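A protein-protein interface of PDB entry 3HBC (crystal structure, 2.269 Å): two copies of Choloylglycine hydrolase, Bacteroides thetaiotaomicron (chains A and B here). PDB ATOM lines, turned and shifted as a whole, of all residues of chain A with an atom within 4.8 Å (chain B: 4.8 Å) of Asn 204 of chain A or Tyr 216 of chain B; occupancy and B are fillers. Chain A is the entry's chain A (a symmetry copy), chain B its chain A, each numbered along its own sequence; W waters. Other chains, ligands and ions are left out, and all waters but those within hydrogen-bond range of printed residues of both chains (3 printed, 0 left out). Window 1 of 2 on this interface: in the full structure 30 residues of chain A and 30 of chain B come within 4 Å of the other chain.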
ATOM      1  N   ALA A   3      -1.982 -15.123  34.090  1.00  0.00           N
ATOM      2  CA  ALA A   3      -2.747 -15.966  33.192  1.00  0.00           C
ATOM      3  C   ALA A   3      -2.918 -17.348  33.807  1.00  0.00           C
ATOM      4  O   ALA A   3      -1.951 -18.010  34.149  1.00  0.00           O
ATOM      5  CB  ALA A   3      -2.046 -16.060  31.826  1.00  0.00           C
ATOM      6  N   GLY A 202      -6.271 -17.183  19.068  1.00  0.00           N
ATOM      7  CA  GLY A 202      -5.106 -17.987  19.433  1.00  0.00           C
ATOM      8  C   GLY A 202      -4.079 -17.319  20.336  1.00  0.00           C
ATOM      9  O   GLY A 202      -2.940 -17.764  20.462  1.00  0.00           O
ATOM     10  N   THR A 203      -4.504 -16.259  20.998  1.00  0.00           N
ATOM     11  CA  THR A 203      -3.627 -15.432  21.804  1.00  0.00           C
ATOM     12  C   THR A 203      -3.543 -15.955  23.261  1.00  0.00           C
ATOM     13  O   THR A 203      -4.258 -16.893  23.623  1.00  0.00           O
ATOM     14  CB  THR A 203      -4.171 -13.990  21.669  1.00  0.00           C
ATOM     15  OG1 THR A 203      -3.253 -13.183  20.925  1.00  0.00           O
ATOM     16  CG2 THR A 203      -4.541 -13.346  22.992  1.00  0.00           C
ATOM     17  N   ASN A 204      -2.664 -15.362  24.074  1.00  0.00           N
ATOM     18  CA  ASN A 204      -2.594 -15.663  25.514  1.00  0.00           C
ATOM     19  C   ASN A 204      -3.577 -14.834  26.367  1.00  0.00           C
ATOM     20  O   ASN A 204      -3.572 -14.922  27.599  1.00  0.00           O
ATOM     21  CB  ASN A 204      -1.166 -15.461  26.043  1.00  0.00           C
ATOM     22  CG  ASN A 204      -0.123 -16.249  25.255  1.00  0.00           C
ATOM     23  OD1 ASN A 204      -0.289 -17.445  24.999  1.00  0.00           O
ATOM     24  ND2 ASN A 204       0.961 -15.573  24.869  1.00  0.00           N
ATOM     25  N   ARG A 205      -4.408 -14.030  25.712  1.00  0.00           N
ATOM     26  CA  ARG A 205      -5.415 -13.201  26.394  1.00  0.00           C
ATOM     27  C   ARG A 205      -6.352 -14.097  27.173  1.00  0.00           C
ATOM     28  O   ARG A 205      -6.665 -15.212  26.742  1.00  0.00           O
ATOM     29  CB  ARG A 205      -6.227 -12.396  25.358  1.00  0.00           C
ATOM     30  CG  ARG A 205      -6.765 -11.042  25.777  1.00  0.00           C
ATOM     31  CD  ARG A 205      -7.035 -10.096  24.571  1.00  0.00           C
ATOM     32  NE  ARG A 205      -7.253 -10.817  23.324  1.00  0.00           N
ATOM     33  CZ  ARG A 205      -6.616 -10.553  22.188  1.00  0.00           C
ATOM     34  NH1 ARG A 205      -5.753  -9.544  22.133  1.00  0.00           N
ATOM     35  NH2 ARG A 205      -6.866 -11.273  21.093  1.00  0.00           N
ATOM     36  N   SER A 206      -6.799 -13.602  28.317  1.00  0.00           N
ATOM     37  CA  SER A 206      -7.716 -14.327  29.187  1.00  0.00           C
ATOM     38  C   SER A 206      -8.914 -14.899  28.448  1.00  0.00           C
ATOM     39  O   SER A 206      -9.230 -16.072  28.620  1.00  0.00           O
ATOM     40  CB  SER A 206      -8.192 -13.425  30.323  1.00  0.00           C
ATOM     41  OG  SER A 206      -9.336 -13.976  30.947  1.00  0.00           O
ATOM     42  N   ARG A 209      -7.971 -17.804  25.848  1.00  0.00           N
ATOM     43  CA  ARG A 209      -7.735 -19.072  26.523  1.00  0.00           C
ATOM     44  C   ARG A 209      -9.076 -19.703  26.925  1.00  0.00           C
ATOM     45  O   ARG A 209      -9.290 -20.903  26.754  1.00  0.00           O
ATOM     46  CB  ARG A 209      -6.802 -18.871  27.712  1.00  0.00           C
ATOM     47  CG  ARG A 209      -5.360 -18.600  27.276  1.00  0.00           C
ATOM     48  CD  ARG A 209      -4.407 -18.424  28.455  1.00  0.00           C
ATOM     49  NE  ARG A 209      -4.518 -17.111  29.089  1.00  0.00           N
ATOM     50  CZ  ARG A 209      -5.132 -16.850  30.241  1.00  0.00           C
ATOM     51  NH1 ARG A 209      -5.728 -17.811  30.959  1.00  0.00           N
ATOM     52  NH2 ARG A 209      -5.136 -15.603  30.682  1.00  0.00           N
ATOM     53  N   SER A 241      -1.739 -22.988  27.464  1.00  0.00           N
ATOM     54  CA  SER A 241      -0.599 -22.477  28.199  1.00  0.00           C
ATOM     55  C   SER A 241       0.012 -21.308  27.460  1.00  0.00           C
ATOM     56  O   SER A 241      -0.238 -21.116  26.271  1.00  0.00           O
ATOM     57  CB  SER A 241       0.446 -23.572  28.407  1.00  0.00           C
ATOM     58  OG  SER A 241      -0.152 -24.633  29.118  1.00  0.00           O
ATOM     59  N   VAL A 242       0.817 -20.528  28.165  1.00  0.00           N
ATOM     60  CA  VAL A 242       1.507 -19.406  27.556  1.00  0.00           C
ATOM     61  C   VAL A 242       2.944 -19.821  27.321  1.00  0.00           C
ATOM     62  O   VAL A 242       3.643 -20.139  28.262  1.00  0.00           O
ATOM     63  CB  VAL A 242       1.498 -18.192  28.491  1.00  0.00           C
ATOM     64  CG1 VAL A 242       2.247 -17.032  27.870  1.00  0.00           C
ATOM     65  CG2 VAL A 242       0.085 -17.812  28.822  1.00  0.00           C
ATOM     66  N   PRO A 243       3.390 -19.825  26.066  1.00  0.00           N
ATOM     67  CA  PRO A 243       4.768 -20.255  25.810  1.00  0.00           C
ATOM     68  C   PRO A 243       5.750 -19.561  26.750  1.00  0.00           C
ATOM     69  O   PRO A 243       5.518 -18.422  27.170  1.00  0.00           O
ATOM     70  CB  PRO A 243       5.006 -19.838  24.362  1.00  0.00           C
ATOM     71  CG  PRO A 243       3.642 -19.836  23.748  1.00  0.00           C
ATOM     72  CD  PRO A 243       2.692 -19.416  24.839  1.00  0.00           C
ATOM     73  N   ILE A 246       7.741 -15.807  27.358  1.00  0.00           N
ATOM     74  CA  ILE A 246       7.158 -14.910  26.366  1.00  0.00           C
ATOM     75  C   ILE A 246       7.266 -13.442  26.782  1.00  0.00           C
ATOM     76  O   ILE A 246       6.629 -12.989  27.738  1.00  0.00           O
ATOM     77  CB  ILE A 246       5.698 -15.307  25.998  1.00  0.00           C
ATOM     78  CG1 ILE A 246       5.656 -15.888  24.587  1.00  0.00           C
ATOM     79  CG2 ILE A 246       4.768 -14.106  26.016  1.00  0.00           C
ATOM     80  CD1 ILE A 246       6.972 -16.481  24.138  1.00  0.00           C
ATOM     81  N   LEU B 200      -3.861 -13.889  16.980  1.00  0.00           N
ATOM     82  CA  LEU B 200      -3.224 -15.021  16.336  1.00  0.00           C
ATOM     83  C   LEU B 200      -4.355 -15.935  15.953  1.00  0.00           C
ATOM     84  O   LEU B 200      -5.325 -16.065  16.706  1.00  0.00           O
ATOM     85  CB  LEU B 200      -2.313 -15.781  17.316  1.00  0.00           C
ATOM     86  CG  LEU B 200      -0.940 -15.181  17.607  1.00  0.00           C
ATOM     87  CD1 LEU B 200      -0.196 -15.948  18.716  1.00  0.00           C
ATOM     88  CD2 LEU B 200      -0.121 -15.110  16.336  1.00  0.00           C
ATOM     89  N   ARG B 212       1.457 -19.117  14.468  1.00  0.00           N
ATOM     90  CA  ARG B 212       1.770 -19.148  15.895  1.00  0.00           C
ATOM     91  C   ARG B 212       3.209 -19.595  16.189  1.00  0.00           C
ATOM     92  O   ARG B 212       3.888 -18.986  17.013  1.00  0.00           O
ATOM     93  CB  ARG B 212       0.777 -20.025  16.643  1.00  0.00           C
ATOM     94  CG  ARG B 212      -0.670 -19.549  16.519  1.00  0.00           C
ATOM     95  CD  ARG B 212      -1.517 -20.097  17.664  1.00  0.00           C
ATOM     96  NE  ARG B 212      -1.419 -21.553  17.838  1.00  0.00           N
ATOM     97  CZ  ARG B 212      -2.122 -22.451  17.149  1.00  0.00           C
ATOM     98  NH1 ARG B 212      -1.983 -23.755  17.413  1.00  0.00           N
ATOM     99  NH2 ARG B 212      -2.967 -22.054  16.192  1.00  0.00           N
ATOM    100  N   ALA B 213       3.672 -20.646  15.510  1.00  0.00           N
ATOM    101  CA  ALA B 213       5.040 -21.116  15.676  1.00  0.00           C
ATOM    102  C   ALA B 213       5.995 -20.015  15.281  1.00  0.00           C
ATOM    103  O   ALA B 213       6.974 -19.748  15.968  1.00  0.00           O
ATOM    104  CB  ALA B 213       5.291 -22.348  14.819  1.00  0.00           C
ATOM    105  N   SER B 214       5.712 -19.372  14.160  1.00  0.00           N
ATOM    106  CA  SER B 214       6.581 -18.302  13.694  1.00  0.00           C
ATOM    107  C   SER B 214       6.591 -17.142  14.696  1.00  0.00           C
ATOM    108  O   SER B 214       7.641 -16.558  14.969  1.00  0.00           O
ATOM    109  CB  SER B 214       6.167 -17.842  12.291  1.00  0.00           C
ATOM    110  OG  SER B 214       6.856 -16.659  11.935  1.00  0.00           O
ATOM    111  N   PHE B 215       5.435 -16.813  15.271  1.00  0.00           N
ATOM    112  CA  PHE B 215       5.403 -15.705  16.216  1.00  0.00           C
ATOM    113  C   PHE B 215       6.133 -16.060  17.526  1.00  0.00           C
ATOM    114  O   PHE B 215       6.997 -15.325  17.987  1.00  0.00           O
ATOM    115  CB  PHE B 215       3.972 -15.272  16.521  1.00  0.00           C
ATOM    116  CG  PHE B 215       3.876 -14.215  17.602  1.00  0.00           C
ATOM    117  CD1 PHE B 215       4.091 -12.871  17.303  1.00  0.00           C
ATOM    118  CD2 PHE B 215       3.576 -14.565  18.918  1.00  0.00           C
ATOM    119  CE1 PHE B 215       4.007 -11.894  18.295  1.00  0.00           C
ATOM    120  CE2 PHE B 215       3.494 -13.594  19.917  1.00  0.00           C
ATOM    121  CZ  PHE B 215       3.704 -12.256  19.595  1.00  0.00           C
ATOM    122  N   TYR B 216       5.784 -17.192  18.118  1.00  0.00           N
ATOM    123  CA  TYR B 216       6.363 -17.570  19.400  1.00  0.00           C
ATOM    124  C   TYR B 216       7.851 -17.930  19.329  1.00  0.00           C
ATOM    125  O   TYR B 216       8.613 -17.603  20.234  1.00  0.00           O
ATOM    126  CB  TYR B 216       5.556 -18.683  20.059  1.00  0.00           C
ATOM    127  CG  TYR B 216       4.219 -18.205  20.602  1.00  0.00           C
ATOM    128  CD1 TYR B 216       4.151 -17.197  21.565  1.00  0.00           C
ATOM    129  CD2 TYR B 216       3.026 -18.754  20.152  1.00  0.00           C
ATOM    130  CE1 TYR B 216       2.921 -16.759  22.063  1.00  0.00           C
ATOM    131  CE2 TYR B 216       1.803 -18.329  20.645  1.00  0.00           C
ATOM    132  CZ  TYR B 216       1.751 -17.327  21.594  1.00  0.00           C
ATOM    133  OH  TYR B 216       0.530 -16.912  22.077  1.00  0.00           O
ATOM    134  N   ILE B 217       8.280 -18.591  18.264  1.00  0.00           N
ATOM    135  CA  ILE B 217       9.690 -18.951  18.191  1.00  0.00           C
ATOM    136  C   ILE B 217      10.579 -17.699  18.239  1.00  0.00           C
ATOM    137  O   ILE B 217      11.727 -17.759  18.675  1.00  0.00           O
ATOM    138  CB  ILE B 217      10.033 -19.809  16.950  1.00  0.00           C
ATOM    139  CG1 ILE B 217      11.196 -20.766  17.274  1.00  0.00           C
ATOM    140  CG2 ILE B 217      10.356 -18.922  15.733  1.00  0.00           C
ATOM    141  CD1 ILE B 217      10.805 -21.930  18.151  1.00  0.00           C
ATOM    142  N   HIS B 218      10.048 -16.566  17.797  1.00  0.00           N
ATOM    143  CA  HIS B 218      10.807 -15.320  17.823  1.00  0.00           C
ATOM    144  C   HIS B 218      10.583 -14.562  19.127  1.00  0.00           C
ATOM    145  O   HIS B 218      11.229 -13.562  19.383  1.00  0.00           O
ATOM    146  CB  HIS B 218      10.405 -14.410  16.663  1.00  0.00           C
ATOM    147  CG  HIS B 218      10.890 -14.871  15.322  1.00  0.00           C
ATOM    148  ND1 HIS B 218      12.161 -14.597  14.858  1.00  0.00           N
ATOM    149  CD2 HIS B 218      10.265 -15.549  14.336  1.00  0.00           C
ATOM    150  CE1 HIS B 218      12.298 -15.099  13.643  1.00  0.00           C
ATOM    151  NE2 HIS B 218      11.167 -15.685  13.302  1.00  0.00           N
ATOM    152  N   ALA B 219       9.644 -15.025  19.937  1.00  0.00           N
ATOM    153  CA  ALA B 219       9.277 -14.309  21.150  1.00  0.00           C
ATOM    154  C   ALA B 219       9.904 -14.919  22.405  1.00  0.00           C
ATOM    155  O   ALA B 219      10.084 -14.242  23.413  1.00  0.00           O
ATOM    156  CB  ALA B 219       7.751 -14.248  21.286  1.00  0.00           C
ATOM    157  N   ILE B 220      10.224 -16.203  22.359  1.00  0.00           N
ATOM    158  CA  ILE B 220      10.888 -16.816  23.500  1.00  0.00           C
ATOM    159  C   ILE B 220      12.252 -16.183  23.729  1.00  0.00           C
ATOM    160  O   ILE B 220      12.840 -15.591  22.815  1.00  0.00           O
ATOM    161  CB  ILE B 220      11.001 -18.348  23.373  1.00  0.00           C
ATOM    162  CG1 ILE B 220      11.693 -18.725  22.072  1.00  0.00           C
ATOM    163  CG2 ILE B 220       9.614 -19.000  23.526  1.00  0.00           C
ATOM    164  CD1 ILE B 220      11.823 -20.223  21.878  1.00  0.00           C
ATOM    165  N   VAL B 236       6.724 -23.834  22.757  1.00  0.00           N
ATOM    166  CA  VAL B 236       6.221 -23.452  21.451  1.00  0.00           C
ATOM    167  C   VAL B 236       5.597 -24.662  20.747  1.00  0.00           C
ATOM    168  O   VAL B 236       4.442 -24.600  20.300  1.00  0.00           O
ATOM    169  CB  VAL B 236       7.287 -22.844  20.572  1.00  0.00           C
ATOM    170  CG1 VAL B 236       6.717 -22.579  19.175  1.00  0.00           C
ATOM    171  CG2 VAL B 236       7.797 -21.560  21.204  1.00  0.00           C
ATOM    172  N   ASN B 239       2.252 -25.398  21.994  1.00  0.00           N
ATOM    173  CA  ASN B 239       1.248 -24.432  21.574  1.00  0.00           C
ATOM    174  C   ASN B 239       0.653 -24.768  20.195  1.00  0.00           C
ATOM    175  O   ASN B 239      -0.504 -24.469  19.918  1.00  0.00           O
ATOM    176  CB  ASN B 239       1.864 -23.039  21.507  1.00  0.00           C
ATOM    177  CG  ASN B 239       0.842 -21.981  21.123  1.00  0.00           C
ATOM    178  OD1 ASN B 239       0.721 -21.622  19.955  1.00  0.00           O
ATOM    179  ND2 ASN B 239       0.069 -21.512  22.104  1.00  0.00           N
HETATM  180  O   HOH W   1       0.021 -13.922  21.903  1.00  0.00           O
HETATM  181  O   HOH W   2       0.572 -23.030  24.670  1.00  0.00           O
HETATM  182  O   HOH W   3      -1.313 -18.529  22.452  1.00  0.00           O
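Gly 202 of chain A touches Arg 212 of chain B (O to CD, 3.9 Å). Gly 202 of chain A touches Tyr 216 of chain B (O to OH, 3.9 Å). Pro 243 of chain A touches Tyr 216 of chain B. Ile 246 of chain A touches Tyr 216 of chain B (CG1 to CD1, 3.6 Å). Ala 219 of chain B touches Ile 246 of chain A. Ile 246 of chain A touches Ile 220 of chain B.
The backbone carbonyl oxygen (O) of Leu 200 of chain B is in hydrogen-bond range of the backbone NH (N) of Gly 202 of chain A. The side-chain hydroxyl of Tyr 216 of chain B lies within hydrogen-bond range of the side-chain amide oxygen of Asn 204 of chain A (3.1 Å).
Printed residues of chain B within 4 Å of Gly 202 of chain A: Leu 200, Arg 212 and Tyr 216. Of the printed residues of chain B, Asn 204 of chain A touches Tyr 216 (3.1 Å). Of the printed residues of chain B, Pro 243 of chain A touches Tyr 216. Of the printed residues of chain A, Leu 200 of chain B touches Gly 202 (2.8 Å). Printed residues of chain A within 4 Å of Arg 212 of chain B: Gly 202. Of the printed residues of chain A, Tyr 216 of chain B touches Gly 202 (3.9 Å), Asn 204 (3.1 Å), Pro 243 (3.5 Å) and Ile 246 (3.6 Å). Of the printed residues of chain A, Ile 220 of chain B touches Ile 246 (3.7 Å). The nearest printed residue of chain B that does not touch Asn 204 of chain A is Asn 239 of chain B (5.0 Å). The nearest printed residue of chain A that does not touch Tyr 216 of chain B is Thr 203 of chain A (4.3 Å).
No position is printed for both chains. Of the 8 pairs that touch across the chains among the printed residues, none has its exchanged pair printed and touching as well.
The backbone carbonyl oxygen (O) of Asn 239 of chain B is in hydrogen-bond range of the guanidinium group (NH1) of Arg 212 of chain B (3.0 Å). The guanidinium group of Arg 209 of chain A is in hydrogen-bond range of the backbone carbonyl oxygen of Asn 204 of chain A.
Water W3 lies within hydrogen-bond range of OH of Tyr 216 of chain B (2.5 Å), O of Gly 202 of chain A (2.7 Å), OD1 of Asn 204 of chain A (3.0 Å) and ND2 of Asn 239 of chain B (3.3 Å). Water W2 bridges O of Ser 241 of chain A (2.6 Å) and ND2 of Asn 239 of chain B (3.0 Å). Water W1 lies within hydrogen-bond range of the side-chain hydroxyl (OH) of Tyr 216 of chain B (3.0 Å) and the side-chain hydroxyl (OG1) of Thr 203 of chain A (3.5 Å).
Hydrophobic or aromatic side chains of chain B within 4 Å of the printed part of chain A: Leu 200, Tyr 216, Ala 219 and Ile 220.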
